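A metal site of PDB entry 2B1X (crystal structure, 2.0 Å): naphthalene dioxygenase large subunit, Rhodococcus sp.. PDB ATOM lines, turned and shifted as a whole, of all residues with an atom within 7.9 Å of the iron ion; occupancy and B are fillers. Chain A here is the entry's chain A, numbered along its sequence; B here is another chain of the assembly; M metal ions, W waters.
A ring nitrogen (NE2) of His 216 lies close to the side-chain amide nitrogen (ND2) of Asn 209, 3.4 Å away. N of His 216 sits at hydrogen-bond distance from OD1 of Asp 213 (2.8 Å).
The nearest printed residue that does not touch the iron ion is Asn 209 (4.4 Å).
NE2 of His 216 is bound to the iron ion, 2.1 Å away. A ring nitrogen (NE2) of His 221 binds the iron ion (2.1 Å). Water W2 is bound to the iron ion, at 2.2 Å. The iron ion is bound by water W1 (2.3 Å). OD2 of Asp 372 is bound to the iron ion (2.3 Å). OD1 of Asp 372 is bound to the iron ion, 2.4 Å away.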
ATOM      1  N   ASN A 209     -11.824 -17.694 -22.040  1.00  0.00           N
ATOM      2  CA  ASN A 209     -12.119 -18.619 -23.112  1.00  0.00           C
ATOM      3  C   ASN A 209     -11.540 -18.161 -24.459  1.00  0.00           C
ATOM      4  O   ASN A 209     -10.860 -18.952 -25.161  1.00  0.00           O
ATOM      5  CB  ASN A 209     -13.640 -18.848 -23.188  1.00  0.00           C
ATOM      6  CG  ASN A 209     -14.032 -19.786 -24.303  1.00  0.00           C
ATOM      7  OD1 ASN A 209     -14.001 -19.401 -25.443  1.00  0.00           O
ATOM      8  ND2 ASN A 209     -14.390 -21.029 -23.980  1.00  0.00           N
ATOM      9  N   PHE A 210     -11.767 -16.899 -24.817  1.00  0.00           N
ATOM     10  CA  PHE A 210     -11.312 -16.403 -26.103  1.00  0.00           C
ATOM     11  C   PHE A 210      -9.833 -16.062 -26.107  1.00  0.00           C
ATOM     12  O   PHE A 210      -9.265 -16.094 -27.160  1.00  0.00           O
ATOM     13  CB  PHE A 210     -12.140 -15.185 -26.614  1.00  0.00           C
ATOM     14  CG  PHE A 210     -13.356 -15.570 -27.397  1.00  0.00           C
ATOM     15  CD1 PHE A 210     -14.467 -16.128 -26.765  1.00  0.00           C
ATOM     16  CD2 PHE A 210     -13.380 -15.432 -28.797  1.00  0.00           C
ATOM     17  CE1 PHE A 210     -15.620 -16.496 -27.484  1.00  0.00           C
ATOM     18  CE2 PHE A 210     -14.525 -15.832 -29.560  1.00  0.00           C
ATOM     19  CZ  PHE A 210     -15.641 -16.374 -28.891  1.00  0.00           C
ATOM     20  N   ASP A 213      -8.303 -20.379 -25.465  1.00  0.00           N
ATOM     21  CA  ASP A 213      -8.886 -21.731 -25.315  1.00  0.00           C
ATOM     22  C   ASP A 213      -9.489 -22.328 -26.593  1.00  0.00           C
ATOM     23  O   ASP A 213     -10.627 -21.997 -26.958  1.00  0.00           O
ATOM     24  CB  ASP A 213      -9.935 -21.684 -24.180  1.00  0.00           C
ATOM     25  CG  ASP A 213     -10.290 -23.082 -23.648  1.00  0.00           C
ATOM     26  OD1 ASP A 213     -10.393 -24.065 -24.406  1.00  0.00           O
ATOM     27  OD2 ASP A 213     -10.488 -23.269 -22.457  1.00  0.00           O
ATOM     28  N   ALA A 214      -8.728 -23.173 -27.264  1.00  0.00           N
ATOM     29  CA  ALA A 214      -9.229 -24.011 -28.326  1.00  0.00           C
ATOM     30  C   ALA A 214      -9.631 -25.386 -27.776  1.00  0.00           C
ATOM     31  O   ALA A 214     -10.526 -26.030 -28.302  1.00  0.00           O
ATOM     32  CB  ALA A 214      -8.162 -24.171 -29.389  1.00  0.00           C
ATOM     33  N   HIS A 216     -11.412 -26.492 -25.422  1.00  0.00           N
ATOM     34  CA  HIS A 216     -12.858 -26.711 -25.132  1.00  0.00           C
ATOM     35  C   HIS A 216     -13.704 -27.170 -26.316  1.00  0.00           C
ATOM     36  O   HIS A 216     -14.756 -27.765 -26.136  1.00  0.00           O
ATOM     37  CB  HIS A 216     -13.502 -25.478 -24.442  1.00  0.00           C
ATOM     38  CG  HIS A 216     -13.929 -24.388 -25.383  1.00  0.00           C
ATOM     39  ND1 HIS A 216     -13.029 -23.585 -26.058  1.00  0.00           N
ATOM     40  CD2 HIS A 216     -15.161 -23.987 -25.792  1.00  0.00           C
ATOM     41  CE1 HIS A 216     -13.695 -22.739 -26.820  1.00  0.00           C
ATOM     42  NE2 HIS A 216     -14.993 -22.950 -26.667  1.00  0.00           N
ATOM     43  N   THR A 217     -13.249 -26.891 -27.510  1.00  0.00           N
ATOM     44  CA  THR A 217     -13.976 -27.276 -28.724  1.00  0.00           C
ATOM     45  C   THR A 217     -14.418 -28.740 -28.677  1.00  0.00           C
ATOM     46  O   THR A 217     -15.596 -29.003 -28.862  1.00  0.00           O
ATOM     47  CB  THR A 217     -13.123 -27.043 -29.954  1.00  0.00           C
ATOM     48  OG1 THR A 217     -12.845 -25.649 -30.084  1.00  0.00           O
ATOM     49  CG2 THR A 217     -13.914 -27.373 -31.241  1.00  0.00           C
ATOM     50  N   THR A 220     -17.112 -29.093 -25.292  1.00  0.00           N
ATOM     51  CA  THR A 220     -18.198 -28.101 -25.304  1.00  0.00           C
ATOM     52  C   THR A 220     -18.972 -28.118 -26.618  1.00  0.00           C
ATOM     53  O   THR A 220     -20.215 -27.984 -26.660  1.00  0.00           O
ATOM     54  CB  THR A 220     -17.656 -26.656 -25.062  1.00  0.00           C
ATOM     55  OG1 THR A 220     -17.074 -26.589 -23.748  1.00  0.00           O
ATOM     56  CG2 THR A 220     -18.822 -25.649 -24.999  1.00  0.00           C
ATOM     57  N   HIS A 221     -18.224 -28.264 -27.703  1.00  0.00           N
ATOM     58  CA  HIS A 221     -18.802 -28.213 -29.029  1.00  0.00           C
ATOM     59  C   HIS A 221     -18.860 -29.559 -29.751  1.00  0.00           C
ATOM     60  O   HIS A 221     -18.901 -29.617 -30.992  1.00  0.00           O
ATOM     61  CB  HIS A 221     -18.074 -27.138 -29.852  1.00  0.00           C
ATOM     62  CG  HIS A 221     -18.123 -25.788 -29.217  1.00  0.00           C
ATOM     63  ND1 HIS A 221     -19.306 -25.228 -28.778  1.00  0.00           N
ATOM     64  CD2 HIS A 221     -17.137 -24.926 -28.863  1.00  0.00           C
ATOM     65  CE1 HIS A 221     -19.045 -24.073 -28.205  1.00  0.00           C
ATOM     66  NE2 HIS A 221     -17.747 -23.862 -28.243  1.00  0.00           N
ATOM     67  N   PHE A 307     -13.477 -16.618 -37.713  1.00  0.00           N
ATOM     68  CA  PHE A 307     -13.629 -18.064 -37.869  1.00  0.00           C
ATOM     69  C   PHE A 307     -14.184 -18.425 -39.238  1.00  0.00           C
ATOM     70  O   PHE A 307     -14.955 -17.666 -39.832  1.00  0.00           O
ATOM     71  CB  PHE A 307     -14.577 -18.654 -36.823  1.00  0.00           C
ATOM     72  CG  PHE A 307     -14.189 -18.421 -35.386  1.00  0.00           C
ATOM     73  CD1 PHE A 307     -15.177 -18.322 -34.427  1.00  0.00           C
ATOM     74  CD2 PHE A 307     -12.857 -18.332 -34.976  1.00  0.00           C
ATOM     75  CE1 PHE A 307     -14.857 -18.113 -33.041  1.00  0.00           C
ATOM     76  CE2 PHE A 307     -12.533 -18.119 -33.612  1.00  0.00           C
ATOM     77  CZ  PHE A 307     -13.544 -18.018 -32.652  1.00  0.00           C
ATOM     78  N   THR A 361     -23.774 -19.998 -35.555  1.00  0.00           N
ATOM     79  CA  THR A 361     -22.693 -20.556 -34.716  1.00  0.00           C
ATOM     80  C   THR A 361     -22.472 -19.776 -33.441  1.00  0.00           C
ATOM     81  O   THR A 361     -22.428 -20.373 -32.350  1.00  0.00           O
ATOM     82  CB  THR A 361     -21.345 -20.732 -35.503  1.00  0.00           C
ATOM     83  OG1 THR A 361     -20.898 -19.466 -35.994  1.00  0.00           O
ATOM     84  CG2 THR A 361     -21.560 -21.595 -36.755  1.00  0.00           C
ATOM     85  N   PHE A 362     -22.358 -18.457 -33.559  1.00  0.00           N
ATOM     86  CA  PHE A 362     -22.094 -17.590 -32.426  1.00  0.00           C
ATOM     87  C   PHE A 362     -23.231 -16.586 -32.199  1.00  0.00           C
ATOM     88  O   PHE A 362     -24.226 -16.598 -32.915  1.00  0.00           O
ATOM     89  CB  PHE A 362     -20.682 -16.954 -32.529  1.00  0.00           C
ATOM     90  CG  PHE A 362     -19.584 -17.941 -32.248  1.00  0.00           C
ATOM     91  CD1 PHE A 362     -19.166 -18.841 -33.234  1.00  0.00           C
ATOM     92  CD2 PHE A 362     -19.026 -18.034 -30.982  1.00  0.00           C
ATOM     93  CE1 PHE A 362     -18.196 -19.805 -32.950  1.00  0.00           C
ATOM     94  CE2 PHE A 362     -18.024 -19.001 -30.679  1.00  0.00           C
ATOM     95  CZ  PHE A 362     -17.624 -19.893 -31.676  1.00  0.00           C
ATOM     96  N   PHE A 368     -22.830 -22.945 -31.236  1.00  0.00           N
ATOM     97  CA  PHE A 368     -21.638 -22.994 -30.392  1.00  0.00           C
ATOM     98  C   PHE A 368     -21.881 -22.182 -29.103  1.00  0.00           C
ATOM     99  O   PHE A 368     -21.807 -22.709 -28.003  1.00  0.00           O
ATOM    100  CB  PHE A 368     -20.392 -22.399 -31.097  1.00  0.00           C
ATOM    101  CG  PHE A 368     -19.799 -23.274 -32.153  1.00  0.00           C
ATOM    102  CD1 PHE A 368     -20.438 -23.460 -33.377  1.00  0.00           C
ATOM    103  CD2 PHE A 368     -18.567 -23.900 -31.942  1.00  0.00           C
ATOM    104  CE1 PHE A 368     -19.878 -24.301 -34.358  1.00  0.00           C
ATOM    105  CE2 PHE A 368     -18.005 -24.715 -32.910  1.00  0.00           C
ATOM    106  CZ  PHE A 368     -18.667 -24.917 -34.117  1.00  0.00           C
ATOM    107  N   GLU A 369     -22.172 -20.879 -29.281  1.00  0.00           N
ATOM    108  CA  GLU A 369     -22.149 -19.948 -28.159  1.00  0.00           C
ATOM    109  C   GLU A 369     -23.199 -20.278 -27.085  1.00  0.00           C
ATOM    110  O   GLU A 369     -22.965 -20.032 -25.911  1.00  0.00           O
ATOM    111  CB  GLU A 369     -22.260 -18.491 -28.601  1.00  0.00           C
ATOM    112  CG  GLU A 369     -21.951 -17.480 -27.501  1.00  0.00           C
ATOM    113  CD  GLU A 369     -21.007 -16.379 -27.972  1.00  0.00           C
ATOM    114  OE1 GLU A 369     -21.409 -15.587 -28.873  1.00  0.00           O
ATOM    115  OE2 GLU A 369     -19.854 -16.292 -27.434  1.00  0.00           O
ATOM    116  N   GLN A 370     -24.328 -20.858 -27.465  1.00  0.00           N
ATOM    117  CA  GLN A 370     -25.313 -21.187 -26.449  1.00  0.00           C
ATOM    118  C   GLN A 370     -24.772 -22.171 -25.410  1.00  0.00           C
ATOM    119  O   GLN A 370     -25.114 -22.058 -24.230  1.00  0.00           O
ATOM    120  CB  GLN A 370     -26.647 -21.640 -27.069  1.00  0.00           C
ATOM    121  CG  GLN A 370     -26.610 -22.985 -27.788  1.00  0.00           C
ATOM    122  CD  GLN A 370     -27.949 -23.262 -28.446  1.00  0.00           C
ATOM    123  OE1 GLN A 370     -28.694 -24.135 -27.981  1.00  0.00           O
ATOM    124  NE2 GLN A 370     -28.262 -22.525 -29.525  1.00  0.00           N
ATOM    125  N   ASP A 371     -23.905 -23.108 -25.814  1.00  0.00           N
ATOM    126  CA  ASP A 371     -23.267 -24.006 -24.848  1.00  0.00           C
ATOM    127  C   ASP A 371     -22.155 -23.366 -24.056  1.00  0.00           C
ATOM    128  O   ASP A 371     -21.950 -23.704 -22.873  1.00  0.00           O
ATOM    129  CB  ASP A 371     -22.688 -25.263 -25.516  1.00  0.00           C
ATOM    130  CG  ASP A 371     -23.758 -26.196 -26.062  1.00  0.00           C
ATOM    131  OD1 ASP A 371     -24.990 -26.048 -25.775  1.00  0.00           O
ATOM    132  OD2 ASP A 371     -23.431 -27.127 -26.793  1.00  0.00           O
ATOM    133  N   ASP A 372     -21.377 -22.490 -24.712  1.00  0.00           N
ATOM    134  CA  ASP A 372     -20.410 -21.660 -24.004  1.00  0.00           C
ATOM    135  C   ASP A 372     -21.082 -20.936 -22.847  1.00  0.00           C
ATOM    136  O   ASP A 372     -20.577 -20.964 -21.710  1.00  0.00           O
ATOM    137  CB  ASP A 372     -19.706 -20.644 -24.944  1.00  0.00           C
ATOM    138  CG  ASP A 372     -18.753 -21.300 -25.901  1.00  0.00           C
ATOM    139  OD1 ASP A 372     -17.893 -22.089 -25.450  1.00  0.00           O
ATOM    140  OD2 ASP A 372     -18.788 -21.117 -27.147  1.00  0.00           O
ATOM    141  N   ALA A 373     -22.236 -20.327 -23.112  1.00  0.00           N
ATOM    142  CA  ALA A 373     -22.964 -19.617 -22.071  1.00  0.00           C
ATOM    143  C   ALA A 373     -23.354 -20.526 -20.904  1.00  0.00           C
ATOM    144  O   ALA A 373     -23.263 -20.131 -19.741  1.00  0.00           O
ATOM    145  CB  ALA A 373     -24.238 -18.907 -22.637  1.00  0.00           C
ATOM    146  N   ASN A 375     -21.927 -23.284 -19.921  1.00  0.00           N
ATOM    147  CA  ASN A 375     -20.740 -23.578 -19.122  1.00  0.00           C
ATOM    148  C   ASN A 375     -20.317 -22.461 -18.154  1.00  0.00           C
ATOM    149  O   ASN A 375     -19.979 -22.722 -17.002  1.00  0.00           O
ATOM    150  CB  ASN A 375     -19.552 -23.955 -20.008  1.00  0.00           C
ATOM    151  CG  ASN A 375     -19.717 -25.337 -20.712  1.00  0.00           C
ATOM    152  OD1 ASN A 375     -20.617 -26.125 -20.406  1.00  0.00           O
ATOM    153  ND2 ASN A 375     -18.866 -25.583 -21.673  1.00  0.00           N
ATOM    154  N   TRP A 376     -20.316 -21.211 -18.630  1.00  0.00           N
ATOM    155  CA  TRP A 376     -19.859 -20.098 -17.798  1.00  0.00           C
ATOM    156  C   TRP A 376     -20.811 -19.851 -16.654  1.00  0.00           C
ATOM    157  O   TRP A 376     -20.364 -19.546 -15.595  1.00  0.00           O
ATOM    158  CB  TRP A 376     -19.606 -18.795 -18.598  1.00  0.00           C
ATOM    159  CG  TRP A 376     -18.661 -19.040 -19.785  1.00  0.00           C
ATOM    160  CD1 TRP A 376     -17.636 -19.947 -19.823  1.00  0.00           C
ATOM    161  CD2 TRP A 376     -18.657 -18.375 -21.064  1.00  0.00           C
ATOM    162  NE1 TRP A 376     -17.030 -19.927 -21.059  1.00  0.00           N
ATOM    163  CE2 TRP A 376     -17.615 -18.952 -21.832  1.00  0.00           C
ATOM    164  CE3 TRP A 376     -19.417 -17.346 -21.642  1.00  0.00           C
ATOM    165  CZ2 TRP A 376     -17.305 -18.541 -23.135  1.00  0.00           C
ATOM    166  CZ3 TRP A 376     -19.140 -16.955 -22.958  1.00  0.00           C
ATOM    167  CH2 TRP A 376     -18.087 -17.523 -23.676  1.00  0.00           C
ATOM    168  N   TYR B 110     -17.181 -28.908 -20.144  1.00  0.00           N
ATOM    169  CA  TYR B 110     -16.351 -27.806 -20.648  1.00  0.00           C
ATOM    170  C   TYR B 110     -15.194 -28.346 -21.528  1.00  0.00           C
ATOM    171  O   TYR B 110     -15.185 -28.104 -22.731  1.00  0.00           O
ATOM    172  CB  TYR B 110     -15.889 -26.905 -19.508  1.00  0.00           C
ATOM    173  CG  TYR B 110     -15.476 -25.487 -19.904  1.00  0.00           C
ATOM    174  CD1 TYR B 110     -15.161 -24.542 -18.921  1.00  0.00           C
ATOM    175  CD2 TYR B 110     -15.390 -25.101 -21.236  1.00  0.00           C
ATOM    176  CE1 TYR B 110     -14.742 -23.260 -19.269  1.00  0.00           C
ATOM    177  CE2 TYR B 110     -14.967 -23.814 -21.596  1.00  0.00           C
ATOM    178  CZ  TYR B 110     -14.650 -22.905 -20.604  1.00  0.00           C
ATOM    179  OH  TYR B 110     -14.257 -21.623 -20.929  1.00  0.00           O
HETATM  180 FE    FE M   1     -16.735 -22.128 -27.511  1.00  0.00          FE
HETATM  181  O   HOH W   1     -16.007 -20.006 -27.097  1.00  0.00           O
HETATM  182  O   HOH W   2     -15.692 -21.735 -29.425  1.00  0.00           O
